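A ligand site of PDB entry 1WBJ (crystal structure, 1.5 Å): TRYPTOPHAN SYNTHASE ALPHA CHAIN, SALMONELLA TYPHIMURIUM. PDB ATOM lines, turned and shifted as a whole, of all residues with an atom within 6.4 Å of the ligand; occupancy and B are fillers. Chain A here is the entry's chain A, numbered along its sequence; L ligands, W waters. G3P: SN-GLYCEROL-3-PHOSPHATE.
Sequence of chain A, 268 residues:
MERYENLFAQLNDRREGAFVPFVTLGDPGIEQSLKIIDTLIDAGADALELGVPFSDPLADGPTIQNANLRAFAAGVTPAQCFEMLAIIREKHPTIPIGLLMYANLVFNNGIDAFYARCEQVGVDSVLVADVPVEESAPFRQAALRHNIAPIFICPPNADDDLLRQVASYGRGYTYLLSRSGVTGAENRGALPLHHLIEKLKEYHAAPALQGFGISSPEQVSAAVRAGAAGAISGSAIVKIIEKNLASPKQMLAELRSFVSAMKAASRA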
ATOM      1  N   PHE A  22      11.837  -0.704   1.929  1.00  0.00           N
ATOM      2  CA  PHE A  22      11.384   0.004   3.117  1.00  0.00           C
ATOM      3  C   PHE A  22       9.850  -0.087   3.258  1.00  0.00           C
ATOM      4  O   PHE A  22       9.123   0.055   2.257  1.00  0.00           O
ATOM      5  CB  PHE A  22      11.789   1.462   3.030  1.00  0.00           C
ATOM      6  CG  PHE A  22      11.098   2.318   4.059  1.00  0.00           C
ATOM      7  CD1 PHE A  22       9.820   2.835   3.844  1.00  0.00           C
ATOM      8  CD2 PHE A  22      11.722   2.582   5.280  1.00  0.00           C
ATOM      9  CE1 PHE A  22       9.195   3.645   4.850  1.00  0.00           C
ATOM     10  CE2 PHE A  22      11.148   3.364   6.264  1.00  0.00           C
ATOM     11  CZ  PHE A  22       9.899   3.880   6.090  1.00  0.00           C
ATOM     12  N   GLU A  49      14.453  -2.244   5.691  1.00  0.00           N
ATOM     13  CA  GLU A  49      14.613  -0.897   6.268  1.00  0.00           C
ATOM     14  C   GLU A  49      13.178  -0.625   6.770  1.00  0.00           C
ATOM     15  O   GLU A  49      12.227  -0.759   5.965  1.00  0.00           O
ATOM     16  CB  GLU A  49      14.978   0.091   5.183  1.00  0.00           C
ATOM     17  CG  GLU A  49      15.395   1.374   5.846  1.00  0.00           C
ATOM     18  CD  GLU A  49      16.914   1.415   5.760  1.00  0.00           C
ATOM     19  OE1 GLU A  49      17.481   0.303   5.710  1.00  0.00           O
ATOM     20  OE2 GLU A  49      17.546   2.472   5.767  1.00  0.00           O
ATOM     21  N   ASP A  60      10.122  12.919   4.583  1.00  0.00           N
ATOM     22  CA  ASP A  60       9.282  12.080   3.718  1.00  0.00           C
ATOM     23  C   ASP A  60       8.312  12.806   2.802  1.00  0.00           C
ATOM     24  O   ASP A  60       7.646  13.740   3.229  1.00  0.00           O
ATOM     25  CB  ASP A  60       8.485  11.043   4.581  1.00  0.00           C
ATOM     26  CG  ASP A  60       9.376   9.947   5.085  1.00  0.00           C
ATOM     27  OD1 ASP A  60       9.932   9.174   4.246  1.00  0.00           O
ATOM     28  OD2 ASP A  60       9.473   9.759   6.353  1.00  0.00           O
ATOM     29  N   ILE A  64       4.994   8.341   1.888  1.00  0.00           N
ATOM     30  CA  ILE A  64       5.300   7.884   3.232  1.00  0.00           C
ATOM     31  C   ILE A  64       4.538   8.719   4.307  1.00  0.00           C
ATOM     32  O   ILE A  64       4.183   8.187   5.359  1.00  0.00           O
ATOM     33  CB  ILE A  64       6.811   7.626   3.423  1.00  0.00           C
ATOM     34  CG1 ILE A  64       7.159   6.372   2.566  1.00  0.00           C
ATOM     35  CG2 ILE A  64       7.097   7.383   4.873  1.00  0.00           C
ATOM     36  CD1 ILE A  64       8.599   6.265   2.323  1.00  0.00           C
ATOM     37  N   LEU A 100      14.709   3.255  10.264  1.00  0.00           N
ATOM     38  CA  LEU A 100      14.930   4.628   9.783  1.00  0.00           C
ATOM     39  C   LEU A 100      14.001   5.411  10.707  1.00  0.00           C
ATOM     40  O   LEU A 100      12.774   5.254  10.686  1.00  0.00           O
ATOM     41  CB  LEU A 100      14.605   4.758   8.268  1.00  0.00           C
ATOM     42  CG  LEU A 100      15.014   6.078   7.603  1.00  0.00           C
ATOM     43  CD1 LEU A 100      14.982   5.959   6.071  1.00  0.00           C
ATOM     44  CD2 LEU A 100      14.164   7.192   8.074  1.00  0.00           C
ATOM     45  N   LEU A 127      19.278   4.429  11.318  1.00  0.00           N
ATOM     46  CA  LEU A 127      19.503   5.728  10.682  1.00  0.00           C
ATOM     47  C   LEU A 127      18.559   6.715  11.305  1.00  0.00           C
ATOM     48  O   LEU A 127      17.379   6.498  11.326  1.00  0.00           O
ATOM     49  CB  LEU A 127      19.176   5.673   9.171  1.00  0.00           C
ATOM     50  CG  LEU A 127      19.178   7.056   8.466  1.00  0.00           C
ATOM     51  CD1 LEU A 127      20.463   7.876   8.613  1.00  0.00           C
ATOM     52  CD2 LEU A 127      18.874   6.843   6.926  1.00  0.00           C
ATOM     53  N   TYR A 175      24.285   5.129   3.721  1.00  0.00           N
ATOM     54  CA  TYR A 175      23.059   5.420   2.944  1.00  0.00           C
ATOM     55  C   TYR A 175      23.417   6.464   1.924  1.00  0.00           C
ATOM     56  O   TYR A 175      23.593   7.623   2.284  1.00  0.00           O
ATOM     57  CB  TYR A 175      21.963   5.904   3.907  1.00  0.00           C
ATOM     58  CG  TYR A 175      20.560   5.877   3.319  1.00  0.00           C
ATOM     59  CD1 TYR A 175      20.285   6.618   2.224  1.00  0.00           C
ATOM     60  CD2 TYR A 175      19.535   5.152   3.949  1.00  0.00           C
ATOM     61  CE1 TYR A 175      18.994   6.642   1.646  1.00  0.00           C
ATOM     62  CE2 TYR A 175      18.264   5.156   3.403  1.00  0.00           C
ATOM     63  CZ  TYR A 175      18.020   5.894   2.244  1.00  0.00           C
ATOM     64  OH  TYR A 175      16.766   5.956   1.659  1.00  0.00           O
ATOM     65  N   ARG A 179      19.618  11.784  -4.482  1.00  0.00           N
ATOM     66  CA  ARG A 179      19.319  13.179  -4.827  1.00  0.00           C
ATOM     67  C   ARG A 179      18.912  13.983  -3.606  1.00  0.00           C
ATOM     68  O   ARG A 179      18.739  13.465  -2.506  1.00  0.00           O
ATOM     69  CB  ARG A 179      18.122  13.187  -5.793  1.00  0.00           C
ATOM     70  CG  ARG A 179      16.884  12.408  -5.217  1.00  0.00           C
ATOM     71  CD  ARG A 179      15.538  12.788  -5.882  1.00  0.00           C
ATOM     72  NE  ARG A 179      14.413  11.943  -5.461  1.00  0.00           N
ATOM     73  CZ  ARG A 179      13.786  12.062  -4.307  1.00  0.00           C
ATOM     74  NH1 ARG A 179      14.150  13.007  -3.438  1.00  0.00           N
ATOM     75  NH2 ARG A 179      12.777  11.229  -4.035  1.00  0.00           N
ATOM     76  N   VAL A 182      12.998  14.924  -0.655  1.00  0.00           N
ATOM     77  CA  VAL A 182      12.483  14.009   0.344  1.00  0.00           C
ATOM     78  C   VAL A 182      12.115  12.679  -0.318  1.00  0.00           C
ATOM     79  O   VAL A 182      12.146  12.583  -1.551  1.00  0.00           O
ATOM     80  CB  VAL A 182      11.211  14.564   1.028  1.00  0.00           C
ATOM     81  CG1 VAL A 182      11.594  15.758   1.889  1.00  0.00           C
ATOM     82  CG2 VAL A 182      10.129  14.921   0.035  1.00  0.00           C
ATOM     83  N   THR A 183      11.717  11.680   0.470  1.00  0.00           N
ATOM     84  CA  THR A 183      11.434  10.380  -0.166  1.00  0.00           C
ATOM     85  C   THR A 183      10.295  10.505  -1.205  1.00  0.00           C
ATOM     86  O   THR A 183       9.387  11.394  -1.107  1.00  0.00           O
ATOM     87  CB  THR A 183      11.074   9.324   0.894  1.00  0.00           C
ATOM     88  OG1 THR A 183       9.895   9.702   1.584  1.00  0.00           O
ATOM     89  CG2 THR A 183      12.204   9.142   1.938  1.00  0.00           C
ATOM     90  N   GLY A 184      10.297   9.607  -2.208  1.00  0.00           N
ATOM     91  CA  GLY A 184       9.186   9.606  -3.180  1.00  0.00           C
ATOM     92  C   GLY A 184       9.642   8.917  -4.439  1.00  0.00           C
ATOM     93  O   GLY A 184      10.751   9.202  -4.949  1.00  0.00           O
ATOM     94  N   ALA A 185       8.766   8.038  -4.931  1.00  0.00           N
ATOM     95  CA  ALA A 185       9.024   7.227  -6.099  1.00  0.00           C
ATOM     96  C   ALA A 185       8.876   8.032  -7.385  1.00  0.00           C
ATOM     97  O   ALA A 185       9.462   7.652  -8.408  1.00  0.00           O
ATOM     98  CB  ALA A 185       8.081   5.992  -6.107  1.00  0.00           C
ATOM     99  N   ASN A 187      10.000  11.111  -8.094  1.00  0.00           N
ATOM    100  CA  ASN A 187      11.274  11.836  -8.338  1.00  0.00           C
ATOM    101  C   ASN A 187      12.565  10.971  -8.356  1.00  0.00           C
ATOM    102  O   ASN A 187      13.073  10.518  -7.326  1.00  0.00           O
ATOM    103  CB  ASN A 187      11.339  12.957  -7.307  1.00  0.00           C
ATOM    104  CG  ASN A 187      12.533  13.868  -7.532  1.00  0.00           C
ATOM    105  OD1 ASN A 187      13.329  13.646  -8.435  1.00  0.00           O
ATOM    106  ND2 ASN A 187      12.674  14.898  -6.687  1.00  0.00           N
ATOM    107  N   GLY A 211      19.677   5.055  -1.998  1.00  0.00           N
ATOM    108  CA  GLY A 211      18.244   5.217  -1.692  1.00  0.00           C
ATOM    109  C   GLY A 211      17.703   6.609  -1.978  1.00  0.00           C
ATOM    110  O   GLY A 211      18.490   7.576  -1.962  1.00  0.00           O
ATOM    111  N   PHE A 212      16.361   6.647  -2.129  1.00  0.00           N
ATOM    112  CA  PHE A 212      15.516   7.794  -2.555  1.00  0.00           C
ATOM    113  C   PHE A 212      15.258   7.678  -4.063  1.00  0.00           C
ATOM    114  O   PHE A 212      16.217   7.689  -4.890  1.00  0.00           O
ATOM    115  CB  PHE A 212      16.095   9.201  -2.262  1.00  0.00           C
ATOM    116  CG  PHE A 212      15.884   9.709  -0.829  1.00  0.00           C
ATOM    117  CD1 PHE A 212      15.988   8.873   0.265  1.00  0.00           C
ATOM    118  CD2 PHE A 212      15.648  11.036  -0.602  1.00  0.00           C
ATOM    119  CE1 PHE A 212      15.834   9.346   1.580  1.00  0.00           C
ATOM    120  CE2 PHE A 212      15.491  11.535   0.693  1.00  0.00           C
ATOM    121  CZ  PHE A 212      15.573  10.699   1.779  1.00  0.00           C
ATOM    122  N   GLY A 213      13.955   7.573  -4.398  1.00  0.00           N
ATOM    123  CA  GLY A 213      13.518   7.545  -5.809  1.00  0.00           C
ATOM    124  C   GLY A 213      13.729   6.204  -6.565  1.00  0.00           C
ATOM    125  O   GLY A 213      13.487   6.176  -7.777  1.00  0.00           O
ATOM    126  N   ILE A 214      14.205   5.125  -5.931  1.00  0.00           N
ATOM    127  CA  ILE A 214      14.487   3.859  -6.636  1.00  0.00           C
ATOM    128  C   ILE A 214      13.187   3.106  -6.768  1.00  0.00           C
ATOM    129  O   ILE A 214      12.642   2.593  -5.734  1.00  0.00           O
ATOM    130  CB  ILE A 214      15.498   2.991  -5.813  1.00  0.00           C
ATOM    131  CG1 ILE A 214      16.843   3.660  -5.606  1.00  0.00           C
ATOM    132  CG2 ILE A 214      15.679   1.610  -6.483  1.00  0.00           C
ATOM    133  CD1 ILE A 214      17.651   3.784  -6.785  1.00  0.00           C
ATOM    134  N   SER A 215      12.659   3.019  -7.989  1.00  0.00           N
ATOM    135  CA  SER A 215      11.372   2.416  -8.169  1.00  0.00           C
ATOM    136  C   SER A 215      11.283   1.401  -9.324  1.00  0.00           C
ATOM    137  O   SER A 215      10.198   0.905  -9.615  1.00  0.00           O
ATOM    138  CB  SER A 215      10.324   3.493  -8.385  1.00  0.00           C
ATOM    139  OG  SER A 215      10.636   4.206  -9.608  1.00  0.00           O
ATOM    140  N   ILE A 232      17.993   0.654  -1.975  1.00  0.00           N
ATOM    141  CA  ILE A 232      16.790   0.649  -1.107  1.00  0.00           C
ATOM    142  C   ILE A 232      15.618   1.256  -1.873  1.00  0.00           C
ATOM    143  O   ILE A 232      15.812   2.313  -2.575  1.00  0.00           O
ATOM    144  CB  ILE A 232      17.066   1.547   0.162  1.00  0.00           C
ATOM    145  CG1 ILE A 232      18.153   0.882   0.990  1.00  0.00           C
ATOM    146  CG2 ILE A 232      15.744   1.733   1.035  1.00  0.00           C
ATOM    147  CD1 ILE A 232      18.809   1.955   2.042  1.00  0.00           C
ATOM    148  N   SER A 233      14.444   0.640  -1.700  1.00  0.00           N
ATOM    149  CA  SER A 233      13.206   1.174  -2.335  1.00  0.00           C
ATOM    150  C   SER A 233      12.085   1.247  -1.313  1.00  0.00           C
ATOM    151  O   SER A 233      11.742   0.223  -0.730  1.00  0.00           O
ATOM    152  CB  SER A 233      12.748   0.227  -3.441  1.00  0.00           C
ATOM    153  OG  SER A 233      11.581   0.725  -4.106  1.00  0.00           O
ATOM    154  N   GLY A 234      11.511   2.430  -1.087  1.00  0.00           N
ATOM    155  CA  GLY A 234      10.484   2.495  -0.061  1.00  0.00           C
ATOM    156  C   GLY A 234       9.159   2.953  -0.631  1.00  0.00           C
ATOM    157  O   GLY A 234       8.183   2.184  -0.638  1.00  0.00           O
ATOM    158  N   SER A 235       9.119   4.207  -1.136  1.00  0.00           N
ATOM    159  CA  SER A 235       7.868   4.703  -1.709  1.00  0.00           C
ATOM    160  C   SER A 235       7.260   3.794  -2.738  1.00  0.00           C
ATOM    161  O   SER A 235       6.032   3.654  -2.807  1.00  0.00           O
ATOM    162  CB  SER A 235       8.082   6.128  -2.321  1.00  0.00           C
ATOM    163  OG  SER A 235       8.344   7.006  -1.244  1.00  0.00           O
ATOM    164  N   ALA A 236       8.085   3.207  -3.577  1.00  0.00           N
ATOM    165  CA  ALA A 236       7.534   2.279  -4.568  1.00  0.00           C
ATOM    166  C   ALA A 236       6.819   1.126  -3.939  1.00  0.00           C
ATOM    167  O   ALA A 236       5.763   0.710  -4.443  1.00  0.00           O
ATOM    168  CB  ALA A 236       8.590   1.792  -5.514  1.00  0.00           C
HETATM  169  O1  G3P L   1      14.942   4.457   2.982  1.00  0.00           O
HETATM  170  C1  G3P L   1      13.671   4.744   2.872  1.00  0.00           C
HETATM  171  C2  G3P L   1      13.216   5.729   1.866  1.00  0.00           C
HETATM  172  O2  G3P L   1      11.778   5.547   2.002  1.00  0.00           O
HETATM  173  C3  G3P L   1      13.644   5.373   0.434  1.00  0.00           C
HETATM  174  O1P G3P L   1      13.341   6.422  -0.504  1.00  0.00           O
HETATM  175  O4P G3P L   1      10.807   6.307  -0.520  1.00  0.00           O
HETATM  176  O2P G3P L   1      12.166   4.929  -2.157  1.00  0.00           O
HETATM  177  O3P G3P L   1      12.178   7.508  -2.309  1.00  0.00           O
HETATM  178  P   G3P L   1      12.035   6.275  -1.433  1.00  0.00           P
HETATM  179  O   HOH W   1      14.666   4.746  -3.118  1.00  0.00           O
HETATM  180  O   HOH W   2      10.688   4.201  -4.191  1.00  0.00           O
HETATM  181  O   HOH W   3      11.298   6.879   4.817  1.00  0.00           O
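Water W2 lies within hydrogen-bond range of an oxygen (O2P) of the ligand (2.6 Å), the backbone NH of Ala 236 (2.9 Å), the backbone carbonyl oxygen of Ile 214 (3.0 Å) and the backbone NH of Ser 235 (3.4 Å).
Water W3 bridges the side-chain carboxylate (OD1) of Asp 60 (2.7 Å) and an oxygen (O2) of the ligand (3.2 Å).
OH of Tyr 175 is in hydrogen-bond range of O1 of the ligand, at 2.7 Å.
The backbone NH (N) of Phe 212 lies close to an oxygen (O1P) of the ligand, at 3.4 Å.
The backbone NH (N) of Gly 234 lies within hydrogen-bond range of an oxygen (O2P) of the ligand (2.8 Å).
OG of Ser 235 is in hydrogen-bond range of O4P of the ligand.
N of Gly 184 sits at hydrogen-bond distance from O3P of the ligand, at 2.8 Å.
An oxygen (O3P) of the ligand is in hydrogen-bond range of the backbone NH (N) of Gly 213 (2.7 Å).
N of Ser 235 sits at hydrogen-bond distance from O4P of the ligand, 2.8 Å away.
Phe 22 touches the ligand.
Ile 64 touches the ligand (CD1 to O2, 3.3 Å).
Leu 100 touches the ligand (CD1 to O1, 3.4 Å).
Thr 183 touches the ligand.
Ile 232 touches the ligand.
C of Ser 233 touches O2P of the ligand (3.8 Å).
Hydrophobic or aromatic side chains that line the ligand: Phe 22, Ile 64, Leu 100, Tyr 175, Phe 212 and Ile 232.
Within 4 Å of the ligand: Phe 22, Ile 64, Leu 100, Tyr 175, Thr 183, Gly 184, Phe 212, Gly 213, Ile 232, Ser 233, Gly 234 and Ser 235.
The side-chain carboxylate (OD1) of Asp 60 is in hydrogen-bond range of the side-chain hydroxyl (OG1) of Thr 183 (2.7 Å).
O of Gly 184 is in hydrogen-bond range of NH2 of Arg 179 (3.0 Å).
The backbone carbonyl oxygen (O) of Ser 233 is in hydrogen-bond range of the backbone NH (N) of Phe 22 (2.8 Å).
The backbone NH (N) of Gly 184 lies close to the side-chain hydroxyl (OG) of Ser 235 (3.4 Å).
OG of Ser 233 sits at hydrogen-bond distance from O of Ile 214 (2.7 Å).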
